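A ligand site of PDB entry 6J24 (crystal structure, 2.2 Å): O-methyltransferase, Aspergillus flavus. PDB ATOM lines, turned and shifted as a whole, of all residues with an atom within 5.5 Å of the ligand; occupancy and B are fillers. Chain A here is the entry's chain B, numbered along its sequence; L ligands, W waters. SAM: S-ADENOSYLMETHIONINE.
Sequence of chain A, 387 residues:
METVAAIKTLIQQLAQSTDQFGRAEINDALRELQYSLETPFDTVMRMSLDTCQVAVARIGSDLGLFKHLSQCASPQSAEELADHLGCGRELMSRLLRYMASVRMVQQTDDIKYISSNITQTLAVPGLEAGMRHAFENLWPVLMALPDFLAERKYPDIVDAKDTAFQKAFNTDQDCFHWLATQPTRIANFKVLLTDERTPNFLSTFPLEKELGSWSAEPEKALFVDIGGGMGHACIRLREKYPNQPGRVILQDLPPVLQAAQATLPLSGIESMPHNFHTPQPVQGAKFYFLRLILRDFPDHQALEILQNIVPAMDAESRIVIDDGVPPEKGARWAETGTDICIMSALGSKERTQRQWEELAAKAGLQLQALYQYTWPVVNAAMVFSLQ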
ATOM      1  N   PHE A 189       3.937  20.754  18.406  1.00  0.00           N
ATOM      2  CA  PHE A 189       3.913  19.375  18.910  1.00  0.00           C
ATOM      3  C   PHE A 189       5.054  19.137  19.883  1.00  0.00           C
ATOM      4  O   PHE A 189       4.898  18.402  20.865  1.00  0.00           O
ATOM      5  CB  PHE A 189       3.991  18.396  17.736  1.00  0.00           C
ATOM      6  CG  PHE A 189       3.759  16.957  18.127  1.00  0.00           C
ATOM      7  CD1 PHE A 189       2.481  16.413  18.086  1.00  0.00           C
ATOM      8  CD2 PHE A 189       4.817  16.150  18.526  1.00  0.00           C
ATOM      9  CE1 PHE A 189       2.258  15.083  18.440  1.00  0.00           C
ATOM     10  CE2 PHE A 189       4.609  14.824  18.896  1.00  0.00           C
ATOM     11  CZ  PHE A 189       3.327  14.292  18.849  1.00  0.00           C
ATOM     12  N   LEU A 193       4.702  17.870  24.048  1.00  0.00           N
ATOM     13  CA  LEU A 193       5.324  16.746  24.739  1.00  0.00           C
ATOM     14  C   LEU A 193       5.866  17.099  26.112  1.00  0.00           C
ATOM     15  O   LEU A 193       6.009  16.203  26.947  1.00  0.00           O
ATOM     16  CB  LEU A 193       6.446  16.165  23.872  1.00  0.00           C
ATOM     17  CG  LEU A 193       6.032  15.362  22.646  1.00  0.00           C
ATOM     18  CD1 LEU A 193       7.267  14.973  21.848  1.00  0.00           C
ATOM     19  CD2 LEU A 193       5.224  14.132  23.067  1.00  0.00           C
ATOM     20  N   ASP A 225      10.325   2.166  28.435  1.00  0.00           N
ATOM     21  CA  ASP A 225       9.265   3.133  28.129  1.00  0.00           C
ATOM     22  C   ASP A 225       9.220   3.356  26.622  1.00  0.00           C
ATOM     23  O   ASP A 225       9.981   4.151  26.077  1.00  0.00           O
ATOM     24  CB  ASP A 225       9.502   4.434  28.900  1.00  0.00           C
ATOM     25  CG  ASP A 225       8.321   5.381  28.830  1.00  0.00           C
ATOM     26  OD1 ASP A 225       7.304   5.005  28.218  1.00  0.00           O
ATOM     27  OD2 ASP A 225       8.417   6.492  29.388  1.00  0.00           O
ATOM     28  N   ILE A 226       8.310   2.665  25.957  1.00  0.00           N
ATOM     29  CA  ILE A 226       8.262   2.599  24.497  1.00  0.00           C
ATOM     30  C   ILE A 226       7.439   3.766  23.972  1.00  0.00           C
ATOM     31  O   ILE A 226       6.228   3.853  24.198  1.00  0.00           O
ATOM     32  CB  ILE A 226       7.674   1.250  24.042  1.00  0.00           C
ATOM     33  CG1 ILE A 226       8.467   0.110  24.680  1.00  0.00           C
ATOM     34  CG2 ILE A 226       7.688   1.167  22.546  1.00  0.00           C
ATOM     35  CD1 ILE A 226       7.872  -1.272  24.463  1.00  0.00           C
ATOM     36  N   GLY A 227       8.100   4.668  23.248  1.00  0.00           N
ATOM     37  CA  GLY A 227       7.451   5.908  22.857  1.00  0.00           C
ATOM     38  C   GLY A 227       7.271   6.844  24.041  1.00  0.00           C
ATOM     39  O   GLY A 227       6.265   7.561  24.117  1.00  0.00           O
ATOM     40  N   GLY A 228       8.238   6.848  24.972  1.00  0.00           N
ATOM     41  CA  GLY A 228       8.112   7.595  26.217  1.00  0.00           C
ATOM     42  C   GLY A 228       8.268   9.087  26.120  1.00  0.00           C
ATOM     43  O   GLY A 228       8.151   9.772  27.132  1.00  0.00           O
ATOM     44  N   GLY A 229       8.520   9.625  24.926  1.00  0.00           N
ATOM     45  CA  GLY A 229       8.516  11.077  24.779  1.00  0.00           C
ATOM     46  C   GLY A 229       9.640  11.684  25.595  1.00  0.00           C
ATOM     47  O   GLY A 229      10.797  11.275  25.481  1.00  0.00           O
ATOM     48  N   HIS A 232       8.825  11.214  31.001  1.00  0.00           N
ATOM     49  CA  HIS A 232       8.204  11.570  32.278  1.00  0.00           C
ATOM     50  C   HIS A 232       7.915  10.338  33.122  1.00  0.00           C
ATOM     51  O   HIS A 232       8.117  10.345  34.340  1.00  0.00           O
ATOM     52  CB  HIS A 232       6.915  12.343  32.044  1.00  0.00           C
ATOM     53  CG  HIS A 232       7.127  13.690  31.448  1.00  0.00           C
ATOM     54  ND1 HIS A 232       6.327  14.205  30.445  1.00  0.00           N
ATOM     55  CD2 HIS A 232       8.058  14.643  31.694  1.00  0.00           C
ATOM     56  CE1 HIS A 232       6.754  15.406  30.105  1.00  0.00           C
ATOM     57  NE2 HIS A 232       7.804  15.698  30.853  1.00  0.00           N
ATOM     58  N   ALA A 233       7.435   9.258  32.497  1.00  0.00           N
ATOM     59  CA  ALA A 233       7.189   8.026  33.242  1.00  0.00           C
ATOM     60  C   ALA A 233       8.490   7.482  33.842  1.00  0.00           C
ATOM     61  O   ALA A 233       8.515   7.059  35.004  1.00  0.00           O
ATOM     62  CB  ALA A 233       6.516   6.989  32.330  1.00  0.00           C
ATOM     63  N   GLN A 251      12.668   4.827  25.285  1.00  0.00           N
ATOM     64  CA  GLN A 251      12.734   4.512  23.864  1.00  0.00           C
ATOM     65  C   GLN A 251      11.846   5.469  23.089  1.00  0.00           C
ATOM     66  O   GLN A 251      10.656   5.589  23.394  1.00  0.00           O
ATOM     67  CB  GLN A 251      12.327   3.057  23.598  1.00  0.00           C
ATOM     68  CG  GLN A 251      13.375   2.034  23.993  1.00  0.00           C
ATOM     69  CD  GLN A 251      12.975   0.614  23.648  1.00  0.00           C
ATOM     70  OE1 GLN A 251      11.825   0.364  23.284  1.00  0.00           O
ATOM     71  NE2 GLN A 251      13.912  -0.322  23.767  1.00  0.00           N
ATOM     72  N   ASP A 252      12.422   6.139  22.097  1.00  0.00           N
ATOM     73  CA  ASP A 252      11.659   7.008  21.210  1.00  0.00           C
ATOM     74  C   ASP A 252      12.522   7.289  19.979  1.00  0.00           C
ATOM     75  O   ASP A 252      13.601   6.711  19.802  1.00  0.00           O
ATOM     76  CB  ASP A 252      11.228   8.294  21.922  1.00  0.00           C
ATOM     77  CG  ASP A 252       9.909   8.852  21.374  1.00  0.00           C
ATOM     78  OD1 ASP A 252       9.809   9.055  20.141  1.00  0.00           O
ATOM     79  OD2 ASP A 252       8.957   9.071  22.153  1.00  0.00           O
ATOM     80  N   LEU A 253      12.031   8.172  19.098  1.00  0.00           N
ATOM     81  CA  LEU A 253      12.771   8.525  17.897  1.00  0.00           C
ATOM     82  C   LEU A 253      13.893   9.526  18.224  1.00  0.00           C
ATOM     83  O   LEU A 253      13.743  10.364  19.125  1.00  0.00           O
ATOM     84  CB  LEU A 253      11.831   9.130  16.848  1.00  0.00           C
ATOM     85  CG  LEU A 253      10.691   8.208  16.398  1.00  0.00           C
ATOM     86  CD1 LEU A 253       9.790   8.901  15.388  1.00  0.00           C
ATOM     87  CD2 LEU A 253      11.263   6.906  15.832  1.00  0.00           C
ATOM     88  N   VAL A 256      13.273  13.247  19.349  1.00  0.00           N
ATOM     89  CA  VAL A 256      12.705  13.611  20.637  1.00  0.00           C
ATOM     90  C   VAL A 256      13.617  13.179  21.795  1.00  0.00           C
ATOM     91  O   VAL A 256      13.597  13.814  22.852  1.00  0.00           O
ATOM     92  CB  VAL A 256      11.266  13.061  20.803  1.00  0.00           C
ATOM     93  CG1 VAL A 256      10.686  12.629  19.451  1.00  0.00           C
ATOM     94  CG2 VAL A 256      11.198  11.956  21.830  1.00  0.00           C
ATOM     95  N   HIS A 274      14.653   4.017  19.082  1.00  0.00           N
ATOM     96  CA  HIS A 274      13.894   2.848  18.689  1.00  0.00           C
ATOM     97  C   HIS A 274      12.570   3.247  18.054  1.00  0.00           C
ATOM     98  O   HIS A 274      11.824   4.070  18.598  1.00  0.00           O
ATOM     99  CB  HIS A 274      13.619   1.931  19.885  1.00  0.00           C
ATOM    100  CG  HIS A 274      12.839   0.697  19.530  1.00  0.00           C
ATOM    101  ND1 HIS A 274      11.686   0.337  20.188  1.00  0.00           N
ATOM    102  CD2 HIS A 274      13.039  -0.247  18.582  1.00  0.00           C
ATOM    103  CE1 HIS A 274      11.212  -0.786  19.671  1.00  0.00           C
ATOM    104  NE2 HIS A 274      12.017  -1.153  18.687  1.00  0.00           N
ATOM    105  N   ASN A 275      12.285   2.643  16.898  1.00  0.00           N
ATOM    106  CA  ASN A 275      10.991   2.772  16.230  1.00  0.00           C
ATOM    107  C   ASN A 275      10.151   1.570  16.647  1.00  0.00           C
ATOM    108  O   ASN A 275      10.489   0.428  16.324  1.00  0.00           O
ATOM    109  CB  ASN A 275      11.181   2.843  14.711  1.00  0.00           C
ATOM    110  CG  ASN A 275       9.864   3.034  13.960  1.00  0.00           C
ATOM    111  OD1 ASN A 275       8.832   2.459  14.304  1.00  0.00           O
ATOM    112  ND2 ASN A 275       9.914   3.847  12.908  1.00  0.00           N
ATOM    113  N   PHE A 276       9.032   1.820  17.339  1.00  0.00           N
ATOM    114  CA  PHE A 276       8.318   0.661  17.884  1.00  0.00           C
ATOM    115  C   PHE A 276       7.548  -0.118  16.820  1.00  0.00           C
ATOM    116  O   PHE A 276       6.828  -1.064  17.181  1.00  0.00           O
ATOM    117  CB  PHE A 276       7.389   1.063  19.042  1.00  0.00           C
ATOM    118  CG  PHE A 276       6.431   2.209  18.723  1.00  0.00           C
ATOM    119  CD1 PHE A 276       5.487   2.110  17.718  1.00  0.00           C
ATOM    120  CD2 PHE A 276       6.432   3.348  19.512  1.00  0.00           C
ATOM    121  CE1 PHE A 276       4.607   3.145  17.454  1.00  0.00           C
ATOM    122  CE2 PHE A 276       5.544   4.381  19.269  1.00  0.00           C
ATOM    123  CZ  PHE A 276       4.629   4.281  18.236  1.00  0.00           C
ATOM    124  N   HIS A 277       7.672   0.223  15.542  1.00  0.00           N
ATOM    125  CA  HIS A 277       7.238  -0.680  14.484  1.00  0.00           C
ATOM    126  C   HIS A 277       8.273  -1.736  14.132  1.00  0.00           C
ATOM    127  O   HIS A 277       8.063  -2.499  13.187  1.00  0.00           O
ATOM    128  CB  HIS A 277       6.879   0.112  13.225  1.00  0.00           C
ATOM    129  CG  HIS A 277       5.718   1.050  13.407  1.00  0.00           C
ATOM    130  ND1 HIS A 277       4.424   0.606  13.620  1.00  0.00           N
ATOM    131  CD2 HIS A 277       5.654   2.394  13.404  1.00  0.00           C
ATOM    132  CE1 HIS A 277       3.622   1.636  13.739  1.00  0.00           C
ATOM    133  NE2 HIS A 277       4.334   2.747  13.609  1.00  0.00           N
ATOM    134  N   ARG A 291       2.343   4.092  27.194  1.00  0.00           N
ATOM    135  CA  ARG A 291       1.392   5.070  27.694  1.00  0.00           C
ATOM    136  C   ARG A 291       0.886   5.918  26.526  1.00  0.00           C
ATOM    137  O   ARG A 291       1.682   6.568  25.834  1.00  0.00           O
ATOM    138  CB  ARG A 291       2.005   5.962  28.779  1.00  0.00           C
ATOM    139  CG  ARG A 291       0.994   6.961  29.344  1.00  0.00           C
ATOM    140  CD  ARG A 291       1.404   7.545  30.689  1.00  0.00           C
ATOM    141  NE  ARG A 291       2.564   8.420  30.599  1.00  0.00           N
ATOM    142  CZ  ARG A 291       3.278   8.830  31.644  1.00  0.00           C
ATOM    143  NH1 ARG A 291       2.940   8.439  32.875  1.00  0.00           N
ATOM    144  NH2 ARG A 291       4.321   9.632  31.464  1.00  0.00           N
ATOM    145  N   LEU A 292      -0.432   5.903  26.313  1.00  0.00           N
ATOM    146  CA  LEU A 292      -1.080   6.694  25.273  1.00  0.00           C
ATOM    147  C   LEU A 292      -0.399   6.487  23.910  1.00  0.00           C
ATOM    148  O   LEU A 292      -0.177   7.434  23.163  1.00  0.00           O
ATOM    149  CB  LEU A 292      -1.108   8.177  25.648  1.00  0.00           C
ATOM    150  CG  LEU A 292      -1.824   8.527  26.956  1.00  0.00           C
ATOM    151  CD1 LEU A 292      -1.457   9.927  27.441  1.00  0.00           C
ATOM    152  CD2 LEU A 292      -3.358   8.378  26.811  1.00  0.00           C
ATOM    153  N   ILE A 293      -0.062   5.238  23.603  1.00  0.00           N
ATOM    154  CA  ILE A 293       0.555   4.935  22.321  1.00  0.00           C
ATOM    155  C   ILE A 293      -0.484   4.251  21.437  1.00  0.00           C
ATOM    156  O   ILE A 293      -0.795   4.722  20.338  1.00  0.00           O
ATOM    157  CB  ILE A 293       1.804   4.040  22.475  1.00  0.00           C
ATOM    158  CG1 ILE A 293       2.850   4.722  23.366  1.00  0.00           C
ATOM    159  CG2 ILE A 293       2.398   3.727  21.111  1.00  0.00           C
ATOM    160  CD1 ILE A 293       3.229   6.105  22.884  1.00  0.00           C
ATOM    161  N   ASP A 296      -3.538   5.659  19.486  1.00  0.00           N
ATOM    162  CA  ASP A 296      -3.311   6.452  18.286  1.00  0.00           C
ATOM    163  C   ASP A 296      -3.276   5.617  17.007  1.00  0.00           C
ATOM    164  O   ASP A 296      -3.004   6.179  15.933  1.00  0.00           O
ATOM    165  CB  ASP A 296      -2.017   7.245  18.424  1.00  0.00           C
ATOM    166  CG  ASP A 296      -2.197   8.524  19.224  1.00  0.00           C
ATOM    167  OD1 ASP A 296      -3.316   8.770  19.713  1.00  0.00           O
ATOM    168  OD2 ASP A 296      -1.226   9.291  19.359  1.00  0.00           O
ATOM    169  N   PHE A 297      -3.565   4.313  17.076  1.00  0.00           N
ATOM    170  CA  PHE A 297      -3.461   3.428  15.927  1.00  0.00           C
ATOM    171  C   PHE A 297      -4.689   2.536  15.803  1.00  0.00           C
ATOM    172  O   PHE A 297      -5.246   2.096  16.823  1.00  0.00           O
ATOM    173  CB  PHE A 297      -2.212   2.531  16.037  1.00  0.00           C
ATOM    174  CG  PHE A 297      -0.908   3.301  16.070  1.00  0.00           C
ATOM    175  CD1 PHE A 297      -0.267   3.659  14.894  1.00  0.00           C
ATOM    176  CD2 PHE A 297      -0.338   3.647  17.284  1.00  0.00           C
ATOM    177  CE1 PHE A 297       0.921   4.359  14.925  1.00  0.00           C
ATOM    178  CE2 PHE A 297       0.857   4.344  17.321  1.00  0.00           C
ATOM    179  CZ  PHE A 297       1.491   4.705  16.139  1.00  0.00           C
HETATM  180  N   SAM L   1       4.304   7.836  26.211  1.00  0.00           N
HETATM  181  CA  SAM L   1       4.271   9.290  26.308  1.00  0.00           C
HETATM  182  C   SAM L   1       3.760   9.753  27.666  1.00  0.00           C
HETATM  183  O   SAM L   1       4.357  10.605  28.319  1.00  0.00           O
HETATM  184  OXT SAM L   1       2.724   9.298  28.147  1.00  0.00           O
HETATM  185  CB  SAM L   1       3.403   9.861  25.190  1.00  0.00           C
HETATM  186  CG  SAM L   1       4.175  10.571  24.098  1.00  0.00           C
HETATM  187  SD  SAM L   1       3.196  10.955  22.612  1.00  0.00           S
HETATM  188  CE  SAM L   1       1.478  10.657  23.130  1.00  0.00           C
HETATM  189  C5' SAM L   1       3.575   9.523  21.576  1.00  0.00           C
HETATM  190  C4' SAM L   1       5.081   9.294  21.500  1.00  0.00           C
HETATM  191  O4' SAM L   1       5.394   8.202  20.660  1.00  0.00           O
HETATM  192  C3' SAM L   1       5.781  10.524  20.924  1.00  0.00           C
HETATM  193  O3' SAM L   1       6.796  10.922  21.806  1.00  0.00           O
HETATM  194  C2' SAM L   1       6.398  10.081  19.617  1.00  0.00           C
HETATM  195  O2' SAM L   1       7.700  10.567  19.440  1.00  0.00           O
HETATM  196  C1' SAM L   1       6.465   8.584  19.816  1.00  0.00           C
HETATM  197  N9  SAM L   1       6.448   7.874  18.536  1.00  0.00           N
HETATM  198  C8  SAM L   1       5.673   8.100  17.438  1.00  0.00           C
HETATM  199  N7  SAM L   1       6.024   7.185  16.502  1.00  0.00           N
HETATM  200  C5  SAM L   1       7.014   6.403  17.004  1.00  0.00           C
HETATM  201  C6  SAM L   1       7.731   5.341  16.494  1.00  0.00           C
HETATM  202  N6  SAM L   1       7.494   4.896  15.268  1.00  0.00           N
HETATM  203  N1  SAM L   1       8.710   4.747  17.281  1.00  0.00           N
HETATM  204  C2  SAM L   1       8.969   5.198  18.560  1.00  0.00           C
HETATM  205  N3  SAM L   1       8.244   6.253  19.061  1.00  0.00           N
HETATM  206  C4  SAM L   1       7.292   6.839  18.288  1.00  0.00           C
HETATM  207  O   HOH W   1       6.921  11.869  28.894  1.00  0.00           O
HETATM  208  O   HOH W   2       5.096   4.978  26.479  1.00  0.00           O
HETATM  209  O   HOH W   3       4.074   6.079  13.923  1.00  0.00           O
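The backbone carbonyl oxygen (O) of Arg 291 is in hydrogen-bond range of a nitrogen (N) of the ligand, 2.9 Å away.
NE of Arg 291 lies within salt-bridge range of OXT of the ligand (2.6 Å).
An oxygen (O2') of the ligand lies within hydrogen-bond range of the side-chain carboxylate (OD1) of Asp 252.
The backbone carbonyl oxygen of Gly 227 is in hydrogen-bond range of a nitrogen (N) of the ligand (2.9 Å).
N6 of the ligand lies within hydrogen-bond range of OD1 of Asn 275 (2.9 Å).
N1 of the ligand lies within hydrogen-bond range of N of Phe 276 (2.9 Å).
The backbone carbonyl oxygen (O) of Asp 252 lies within hydrogen-bond range of the backbone NH (N) of His 274.
The side-chain carboxylate (OD2) of Asp 252 sits at hydrogen-bond distance from the backbone NH (N) of Gly 229.
N of Gly 227 is in hydrogen-bond range of O of Gln 251.
The side-chain amide oxygen (OD1) of Asn 275 is in hydrogen-bond range of the backbone NH (N) of His 277.
A ring nitrogen (ND1) of His 274 lies within hydrogen-bond range of the side-chain amide oxygen (OE1) of Gln 251 (3.1 Å).
O of Gln 251 is in hydrogen-bond range of N of Gly 228 (3.1 Å).
The backbone carbonyl oxygen of His 274 lies close to a nitrogen (N1) of the ligand (3.4 Å).
Leu 193 touches the ligand (CD2 to O3', 3.8 Å).
CA of Gly 228 touches N of the ligand (3.8 Å).
CA of Gly 229 touches O3' of the ligand, at 3.4 Å.
Leu 253 touches the ligand.
CG1 of Val 256 touches O2' of the ligand (3.6 Å).
His 277 touches the ligand (CD2 to N6, 3.6 Å).
Leu 292 touches the ligand (O to CE, 3.6 Å).
Ile 293 touches the ligand (CD1 to C5', 3.7 Å).
Hydrophobic or aromatic side chains that line the ligand: Leu 193, Leu 253, Val 256, Phe 276, His 277 and Ile 293.
14 residues have an atom within 4 Å of the ligand: Leu 193, Gly 227, Gly 228, Gly 229, Asp 252, Leu 253, Val 256, His 274, Asn 275, Phe 276, His 277, Arg 291, Leu 292 and Ile 293.
The nearest printed residue that does not touch the ligand is Asp 225 (4.6 Å).
Water W1 lies within hydrogen-bond range of ND1 of His 232 (2.9 Å), O of the ligand (2.9 Å) and O of Gly 228 (3.0 Å).
Water W2 lies within hydrogen-bond range of the backbone carbonyl oxygen (O) of Ile 226 (2.8 Å), the side-chain carboxylate (OD1) of Asp 225 (2.8 Å), a nitrogen (N) of the ligand (3.0 Å) and the backbone NH (N) of Arg 291 (3.0 Å).
Water W3 lies within hydrogen-bond range of a ring nitrogen (NE2) of His 277 (3.4 Å) and a nitrogen (N7) of the ligand (3.4 Å).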
